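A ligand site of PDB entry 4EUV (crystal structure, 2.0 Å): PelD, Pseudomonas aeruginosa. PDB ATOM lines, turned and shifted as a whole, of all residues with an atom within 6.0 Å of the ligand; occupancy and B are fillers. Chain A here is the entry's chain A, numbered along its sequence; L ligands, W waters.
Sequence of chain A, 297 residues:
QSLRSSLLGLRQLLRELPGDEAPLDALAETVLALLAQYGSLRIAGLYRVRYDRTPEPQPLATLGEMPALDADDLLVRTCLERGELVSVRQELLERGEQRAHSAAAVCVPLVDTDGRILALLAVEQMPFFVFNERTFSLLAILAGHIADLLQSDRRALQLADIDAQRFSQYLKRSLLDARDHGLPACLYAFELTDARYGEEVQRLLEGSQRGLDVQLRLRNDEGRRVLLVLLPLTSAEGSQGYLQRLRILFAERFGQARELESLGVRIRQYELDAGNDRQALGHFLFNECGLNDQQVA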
ATOM      1  N   GLN A   1      20.850  10.617 -14.600  1.00  0.00           N
ATOM      2  CA  GLN A   1      21.778  11.770 -14.818  1.00  0.00           C
ATOM      3  C   GLN A   1      23.089  11.357 -15.463  1.00  0.00           C
ATOM      4  O   GLN A   1      23.527  10.197 -15.373  1.00  0.00           O
ATOM      5  CB  GLN A   1      22.130  12.457 -13.488  1.00  0.00           C
ATOM      6  CG  GLN A   1      21.075  13.348 -12.904  1.00  0.00           C
ATOM      7  CD  GLN A   1      21.044  13.222 -11.388  1.00  0.00           C
ATOM      8  OE1 GLN A   1      20.132  12.625 -10.833  1.00  0.00           O
ATOM      9  NE2 GLN A   1      22.055  13.766 -10.710  1.00  0.00           N
ATOM     10  N   ARG A   4      26.012   9.909 -12.705  1.00  0.00           N
ATOM     11  CA  ARG A   4      26.418   8.495 -12.715  1.00  0.00           C
ATOM     12  C   ARG A   4      27.381   8.252 -13.868  1.00  0.00           C
ATOM     13  O   ARG A   4      28.488   7.757 -13.667  1.00  0.00           O
ATOM     14  CB  ARG A   4      25.206   7.545 -12.839  1.00  0.00           C
ATOM     15  CG  ARG A   4      24.381   7.292 -11.559  1.00  0.00           C
ATOM     16  CD  ARG A   4      23.441   6.085 -11.701  1.00  0.00           C
ATOM     17  NE  ARG A   4      22.437   6.208 -12.781  1.00  0.00           N
ATOM     18  CZ  ARG A   4      21.139   6.437 -12.590  1.00  0.00           C
ATOM     19  NH1 ARG A   4      20.640   6.571 -11.351  1.00  0.00           N
ATOM     20  NH2 ARG A   4      20.319   6.552 -13.628  1.00  0.00           N
ATOM     21  N   SER A 208      24.691  -9.692 -13.487  1.00  0.00           N
ATOM     22  CA  SER A 208      23.814  -8.543 -13.711  1.00  0.00           C
ATOM     23  C   SER A 208      24.403  -7.182 -13.270  1.00  0.00           C
ATOM     24  O   SER A 208      23.829  -6.122 -13.561  1.00  0.00           O
ATOM     25  CB  SER A 208      22.450  -8.724 -13.030  1.00  0.00           C
ATOM     26  OG  SER A 208      22.504  -8.472 -11.636  1.00  0.00           O
ATOM     27  N   GLN A 209      25.537  -7.217 -12.579  1.00  0.00           N
ATOM     28  CA  GLN A 209      26.073  -5.986 -11.983  1.00  0.00           C
ATOM     29  C   GLN A 209      26.359  -4.934 -13.040  1.00  0.00           C
ATOM     30  O   GLN A 209      26.939  -5.218 -14.081  1.00  0.00           O
ATOM     31  CB  GLN A 209      27.301  -6.263 -11.127  1.00  0.00           C
ATOM     32  CG  GLN A 209      27.793  -5.037 -10.397  1.00  0.00           C
ATOM     33  CD  GLN A 209      29.130  -5.262  -9.742  1.00  0.00           C
ATOM     34  OE1 GLN A 209      29.252  -6.067  -8.831  1.00  0.00           O
ATOM     35  NE2 GLN A 209      30.149  -4.559 -10.230  1.00  0.00           N
ATOM     36  N   ARG A 210      25.913  -3.717 -12.782  1.00  0.00           N
ATOM     37  CA  ARG A 210      25.987  -2.656 -13.772  1.00  0.00           C
ATOM     38  C   ARG A 210      26.474  -1.376 -13.133  1.00  0.00           C
ATOM     39  O   ARG A 210      26.092  -1.040 -12.009  1.00  0.00           O
ATOM     40  CB  ARG A 210      24.615  -2.441 -14.408  1.00  0.00           C
ATOM     41  CG  ARG A 210      24.616  -1.525 -15.589  1.00  0.00           C
ATOM     42  CD  ARG A 210      23.196  -1.227 -16.082  1.00  0.00           C
ATOM     43  NE  ARG A 210      22.788  -2.149 -17.132  1.00  0.00           N
ATOM     44  CZ  ARG A 210      21.633  -2.076 -17.809  1.00  0.00           C
ATOM     45  NH1 ARG A 210      20.701  -1.144 -17.546  1.00  0.00           N
ATOM     46  NH2 ARG A 210      21.416  -2.987 -18.732  1.00  0.00           N
ATOM     47  N   GLY A 211      27.283  -0.650 -13.896  1.00  0.00           N
ATOM     48  CA  GLY A 211      27.975   0.562 -13.488  1.00  0.00           C
ATOM     49  C   GLY A 211      28.019   1.070 -12.070  1.00  0.00           C
ATOM     50  O   GLY A 211      27.189   1.835 -11.677  1.00  0.00           O
ATOM     51  N   ASP A 213      27.003   0.074  -9.189  1.00  0.00           N
ATOM     52  CA  ASP A 213      26.430  -0.824  -8.173  1.00  0.00           C
ATOM     53  C   ASP A 213      27.572  -1.691  -7.699  1.00  0.00           C
ATOM     54  O   ASP A 213      28.468  -2.004  -8.469  1.00  0.00           O
ATOM     55  CB  ASP A 213      25.349  -1.718  -8.788  1.00  0.00           C
ATOM     56  CG  ASP A 213      24.085  -0.942  -9.157  1.00  0.00           C
ATOM     57  OD1 ASP A 213      24.058   0.317  -9.039  1.00  0.00           O
ATOM     58  OD2 ASP A 213      23.128  -1.590  -9.583  1.00  0.00           O
ATOM     59  N   LEU A 231      22.871   0.027  -4.728  1.00  0.00           N
ATOM     60  CA  LEU A 231      22.715   0.883  -5.875  1.00  0.00           C
ATOM     61  C   LEU A 231      22.860   2.351  -5.473  1.00  0.00           C
ATOM     62  O   LEU A 231      21.879   2.986  -5.036  1.00  0.00           O
ATOM     63  CB  LEU A 231      21.350   0.691  -6.577  1.00  0.00           C
ATOM     64  CG  LEU A 231      20.464  -0.564  -6.496  1.00  0.00           C
ATOM     65  CD1 LEU A 231      19.751  -0.867  -7.812  1.00  0.00           C
ATOM     66  CD2 LEU A 231      21.104  -1.800  -5.929  1.00  0.00           C
ATOM     67  N   PRO A 232      24.080   2.903  -5.607  1.00  0.00           N
ATOM     68  CA  PRO A 232      24.289   4.336  -5.369  1.00  0.00           C
ATOM     69  C   PRO A 232      23.453   5.180  -6.316  1.00  0.00           C
ATOM     70  O   PRO A 232      23.205   4.791  -7.472  1.00  0.00           O
ATOM     71  CB  PRO A 232      25.759   4.554  -5.723  1.00  0.00           C
ATOM     72  CG  PRO A 232      26.405   3.179  -5.603  1.00  0.00           C
ATOM     73  CD  PRO A 232      25.336   2.218  -6.033  1.00  0.00           C
ATOM     74  N   THR A 234      20.494   6.053  -6.786  1.00  0.00           N
ATOM     75  CA  THR A 234      19.382   5.388  -7.454  1.00  0.00           C
ATOM     76  C   THR A 234      18.089   5.666  -6.705  1.00  0.00           C
ATOM     77  O   THR A 234      17.985   5.339  -5.555  1.00  0.00           O
ATOM     78  CB  THR A 234      19.701   3.877  -7.474  1.00  0.00           C
ATOM     79  OG1 THR A 234      20.862   3.674  -8.293  1.00  0.00           O
ATOM     80  CG2 THR A 234      18.515   3.046  -7.984  1.00  0.00           C
ATOM     81  N   GLU A 237      12.217   5.081  -8.277  1.00  0.00           N
ATOM     82  CA  GLU A 237      12.014   4.811  -9.681  1.00  0.00           C
ATOM     83  C   GLU A 237      13.341   4.200 -10.096  1.00  0.00           C
ATOM     84  O   GLU A 237      14.420   4.531  -9.609  1.00  0.00           O
ATOM     85  CB  GLU A 237      11.716   6.097 -10.459  1.00  0.00           C
ATOM     86  CG  GLU A 237      12.393   7.350  -9.863  1.00  0.00           C
ATOM     87  CD  GLU A 237      11.477   8.185  -8.921  1.00  0.00           C
ATOM     88  OE1 GLU A 237      11.553   8.024  -7.662  1.00  0.00           O
ATOM     89  OE2 GLU A 237      10.703   9.016  -9.461  1.00  0.00           O
ATOM     90  N   GLY A 238      13.399   3.259 -10.969  1.00  0.00           N
ATOM     91  CA  GLY A 238      14.852   2.980 -11.045  1.00  0.00           C
ATOM     92  C   GLY A 238      15.300   1.825 -10.185  1.00  0.00           C
ATOM     93  O   GLY A 238      15.803   0.928 -10.776  1.00  0.00           O
ATOM     94  N   SER A 239      15.130   1.819  -8.841  1.00  0.00           N
ATOM     95  CA  SER A 239      15.301   0.541  -8.087  1.00  0.00           C
ATOM     96  C   SER A 239      14.269  -0.381  -8.688  1.00  0.00           C
ATOM     97  O   SER A 239      14.460  -1.586  -8.751  1.00  0.00           O
ATOM     98  CB  SER A 239      14.955   0.580  -6.586  1.00  0.00           C
ATOM     99  OG  SER A 239      15.299   1.774  -5.929  1.00  0.00           O
ATOM    100  N   GLN A 240      13.143   0.186  -9.068  1.00  0.00           N
ATOM    101  CA  GLN A 240      12.100  -0.584  -9.705  1.00  0.00           C
ATOM    102  C   GLN A 240      12.447  -0.955 -11.121  1.00  0.00           C
ATOM    103  O   GLN A 240      12.216  -2.074 -11.529  1.00  0.00           O
ATOM    104  CB  GLN A 240      10.768   0.129  -9.605  1.00  0.00           C
ATOM    105  CG  GLN A 240      10.244   0.115  -8.140  1.00  0.00           C
ATOM    106  CD  GLN A 240       9.799  -1.275  -7.646  1.00  0.00           C
ATOM    107  OE1 GLN A 240      10.027  -1.634  -6.481  1.00  0.00           O
ATOM    108  NE2 GLN A 240       9.118  -2.042  -8.519  1.00  0.00           N
ATOM    109  N   GLY A 241      13.061  -0.026 -11.849  1.00  0.00           N
ATOM    110  CA  GLY A 241      13.628  -0.356 -13.147  1.00  0.00           C
ATOM    111  C   GLY A 241      14.661  -1.476 -13.040  1.00  0.00           C
ATOM    112  O   GLY A 241      14.734  -2.352 -13.913  1.00  0.00           O
ATOM    113  N   TYR A 242      15.448  -1.461 -11.973  1.00  0.00           N
ATOM    114  CA  TYR A 242      16.445  -2.544 -11.759  1.00  0.00           C
ATOM    115  C   TYR A 242      15.783  -3.930 -11.625  1.00  0.00           C
ATOM    116  O   TYR A 242      16.193  -4.917 -12.279  1.00  0.00           O
ATOM    117  CB  TYR A 242      17.294  -2.207 -10.538  1.00  0.00           C
ATOM    118  CG  TYR A 242      18.190  -3.308  -9.976  1.00  0.00           C
ATOM    119  CD1 TYR A 242      19.303  -3.764 -10.694  1.00  0.00           C
ATOM    120  CD2 TYR A 242      17.940  -3.861  -8.727  1.00  0.00           C
ATOM    121  CE1 TYR A 242      20.139  -4.727 -10.201  1.00  0.00           C
ATOM    122  CE2 TYR A 242      18.768  -4.859  -8.214  1.00  0.00           C
ATOM    123  CZ  TYR A 242      19.875  -5.255  -8.954  1.00  0.00           C
ATOM    124  OH  TYR A 242      20.733  -6.208  -8.479  1.00  0.00           O
ATOM    125  N   LEU A 243      14.738  -4.004 -10.806  1.00  0.00           N
ATOM    126  CA  LEU A 243      14.105  -5.291 -10.553  1.00  0.00           C
ATOM    127  C   LEU A 243      13.353  -5.747 -11.805  1.00  0.00           C
ATOM    128  O   LEU A 243      13.255  -6.952 -12.078  1.00  0.00           O
ATOM    129  CB  LEU A 243      13.159  -5.230  -9.368  1.00  0.00           C
ATOM    130  CG  LEU A 243      12.673  -6.493  -8.647  1.00  0.00           C
ATOM    131  CD1 LEU A 243      13.592  -7.716  -8.712  1.00  0.00           C
ATOM    132  CD2 LEU A 243      12.461  -6.088  -7.233  1.00  0.00           C
ATOM    133  N   ARG A 245      14.404  -5.200 -14.754  1.00  0.00           N
ATOM    134  CA  ARG A 245      15.467  -5.689 -15.637  1.00  0.00           C
ATOM    135  C   ARG A 245      15.828  -7.090 -15.197  1.00  0.00           C
ATOM    136  O   ARG A 245      15.972  -7.994 -16.009  1.00  0.00           O
ATOM    137  CB  ARG A 245      16.700  -4.763 -15.557  1.00  0.00           C
ATOM    138  CG  ARG A 245      17.802  -5.147 -16.593  1.00  0.00           C
ATOM    139  CD  ARG A 245      18.882  -4.081 -16.647  1.00  0.00           C
ATOM    140  NE  ARG A 245      19.761  -4.046 -15.460  1.00  0.00           N
ATOM    141  CZ  ARG A 245      20.770  -4.870 -15.232  1.00  0.00           C
ATOM    142  NH1 ARG A 245      21.025  -5.870 -16.094  1.00  0.00           N
ATOM    143  NH2 ARG A 245      21.531  -4.714 -14.153  1.00  0.00           N
HETATM  144  P1  LIG L   1      16.809  -0.377 -18.416  1.00  0.00           P
HETATM  145  O1  LIG L   1      15.415  -0.860 -18.626  1.00  0.00           O
HETATM  146  O2  LIG L   1      17.914  -1.415 -18.380  1.00  0.00           O
HETATM  147  O3  LIG L   1      16.782   0.467 -17.066  1.00  0.00           O
HETATM  148  C1  LIG L   1      15.663   1.287 -16.708  1.00  0.00           C
HETATM  149  C2  LIG L   1      16.095   2.059 -15.478  1.00  0.00           C
HETATM  150  O4  LIG L   1      16.101   1.142 -14.361  1.00  0.00           O
HETATM  151  C3  LIG L   1      17.506   2.624 -15.559  1.00  0.00           C
HETATM  152  O5  LIG L   1      17.583   3.964 -16.045  1.00  0.00           O
HETATM  153  C4  LIG L   1      17.938   2.645 -14.106  1.00  0.00           C
HETATM  154  O6  LIG L   1      17.482   3.818 -13.432  1.00  0.00           O
HETATM  155  C5  LIG L   1      17.234   1.435 -13.529  1.00  0.00           C
HETATM  156  N1  LIG L   1      18.189   0.300 -13.566  1.00  0.00           N
HETATM  157  C6  LIG L   1      18.139  -0.761 -14.383  1.00  0.00           C
HETATM  158  N2  LIG L   1      19.155  -1.611 -14.125  1.00  0.00           N
HETATM  159  C7  LIG L   1      19.873  -1.088 -13.122  1.00  0.00           C
HETATM  160  C8  LIG L   1      21.086  -1.497 -12.378  1.00  0.00           C
HETATM  161  O7  LIG L   1      21.681  -2.678 -12.714  1.00  0.00           O
HETATM  162  N3  LIG L   1      21.527  -0.685 -11.411  1.00  0.00           N
HETATM  163  C9  LIG L   1      20.911   0.515 -11.100  1.00  0.00           C
HETATM  164  N4  LIG L   1      21.429   1.274 -10.118  1.00  0.00           N
HETATM  165  N5  LIG L   1      19.776   0.952 -11.731  1.00  0.00           N
HETATM  166  C10 LIG L   1      19.251   0.194 -12.760  1.00  0.00           C
HETATM  167  P2  LIG L   1      18.898   4.499 -16.819  1.00  0.00           P
HETATM  168  O8  LIG L   1      18.529   5.905 -17.254  1.00  0.00           O
HETATM  169  O9  LIG L   1      20.120   4.309 -15.954  1.00  0.00           O
HETATM  170  O10 LIG L   1      19.035   3.552 -18.103  1.00  0.00           O
HETATM  171  C11 LIG L   1      18.153   3.724 -19.215  1.00  0.00           C
HETATM  172  C12 LIG L   1      18.436   2.658 -20.263  1.00  0.00           C
HETATM  173  O11 LIG L   1      19.750   2.810 -20.763  1.00  0.00           O
HETATM  174  C13 LIG L   1      18.450   1.245 -19.707  1.00  0.00           C
HETATM  175  O12 LIG L   1      17.145   0.685 -19.585  1.00  0.00           O
HETATM  176  C14 LIG L   1      19.332   0.471 -20.655  1.00  0.00           C
HETATM  177  O13 LIG L   1      18.624   0.116 -21.862  1.00  0.00           O
HETATM  178  C15 LIG L   1      20.357   1.531 -20.998  1.00  0.00           C
HETATM  179  N6  LIG L   1      21.532   1.414 -20.092  1.00  0.00           N
HETATM  180  C16 LIG L   1      21.837   2.169 -19.011  1.00  0.00           C
HETATM  181  N7  LIG L   1      23.001   1.765 -18.464  1.00  0.00           N
HETATM  182  C17 LIG L   1      23.460   0.750 -19.214  1.00  0.00           C
HETATM  183  C18 LIG L   1      24.632  -0.150 -19.229  1.00  0.00           C
HETATM  184  O14 LIG L   1      25.612  -0.065 -18.306  1.00  0.00           O
HETATM  185  N8  LIG L   1      24.697  -1.093 -20.183  1.00  0.00           N
HETATM  186  C19 LIG L   1      23.766  -1.229 -21.149  1.00  0.00           C
HETATM  187  N9  LIG L   1      23.930  -2.189 -22.089  1.00  0.00           N
HETATM  188  N10 LIG L   1      22.656  -0.447 -21.211  1.00  0.00           N
HETATM  189  C20 LIG L   1      22.478   0.537 -20.289  1.00  0.00           C
HETATM  190  O   HOH W   1      23.695  -3.833 -10.985  1.00  0.00           O
HETATM  191  O   HOH W   2      24.187   3.066  -9.414  1.00  0.00           O
HETATM  192  O   HOH W   3      19.319   3.931 -11.379  1.00  0.00           O
HETATM  193  O   HOH W   4      21.170   1.575 -15.281  1.00  0.00           O
HETATM  194  O   HOH W   5      19.670  -3.057 -20.389  1.00  0.00           O
HETATM  195  O   HOH W   6      13.884  -1.990 -16.558  1.00  0.00           O
HETATM  196  O   HOH W   7      15.317   5.144 -14.041  1.00  0.00           O
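CD1 of Leu 231 touches N4 of the ligand, 3.6 Å away. Gly 238 touches the ligand. Gly 241 touches the ligand. CD1 of Tyr 242 touches O7 of the ligand, 3.3 Å away. Hydrophobic or aromatic side chains that line the ligand: Leu 231 and Tyr 242. Within 4 Å of the ligand: Arg 4, Arg 210, Asp 213, Leu 231, Thr 234, Gly 238, Gly 241, Tyr 242 and Arg 245.
The backbone carbonyl oxygen (O) of Ser 208 lies within hydrogen-bond range of the guanidinium group (NH2) of Arg 245 (2.8 Å). The side-chain hydroxyl (OG1) of Thr 234 sits close to the backbone carbonyl oxygen (O) of Leu 231 (3.5 Å). The side-chain hydroxyl (OG1) of Thr 234 is in hydrogen-bond range of the backbone carbonyl oxygen (O) of Pro 232.
NH2 of Arg 245 sits at hydrogen-bond distance from O7 of the ligand (2.5 Å). N3 of the ligand lies within hydrogen-bond range of OD2 of Asp 213, 2.6 Å away. The guanidinium group (NH1) of Arg 210 lies within salt-bridge range of an oxygen (O2) of the ligand (2.9 Å). The side-chain hydroxyl (OG1) of Thr 234 is in hydrogen-bond range of a nitrogen (N4) of the ligand, 3.1 Å away. NH2 of Arg 4 is in salt-bridge range of O9 of the ligand, at 3.2 Å.
Water W3 lies within hydrogen-bond range of O6 of the ligand (2.8 Å), NH1 of Arg 4 (3.0 Å) and OG1 of Thr 234 (3.5 Å). Water W6 lies within hydrogen-bond range of the backbone carbonyl oxygen of Gly 241 (2.8 Å) and an oxygen (O1) of the ligand (2.8 Å). Water W5 lies within hydrogen-bond range of the guanidinium group (NH2) of Arg 210 (2.4 Å) and an oxygen (O2) of the ligand (3.1 Å). Water W2 lies within hydrogen-bond range of O of Pro 232 (2.8 Å), OD1 of Asp 213 (2.8 Å) and N4 of the ligand (3.4 Å).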
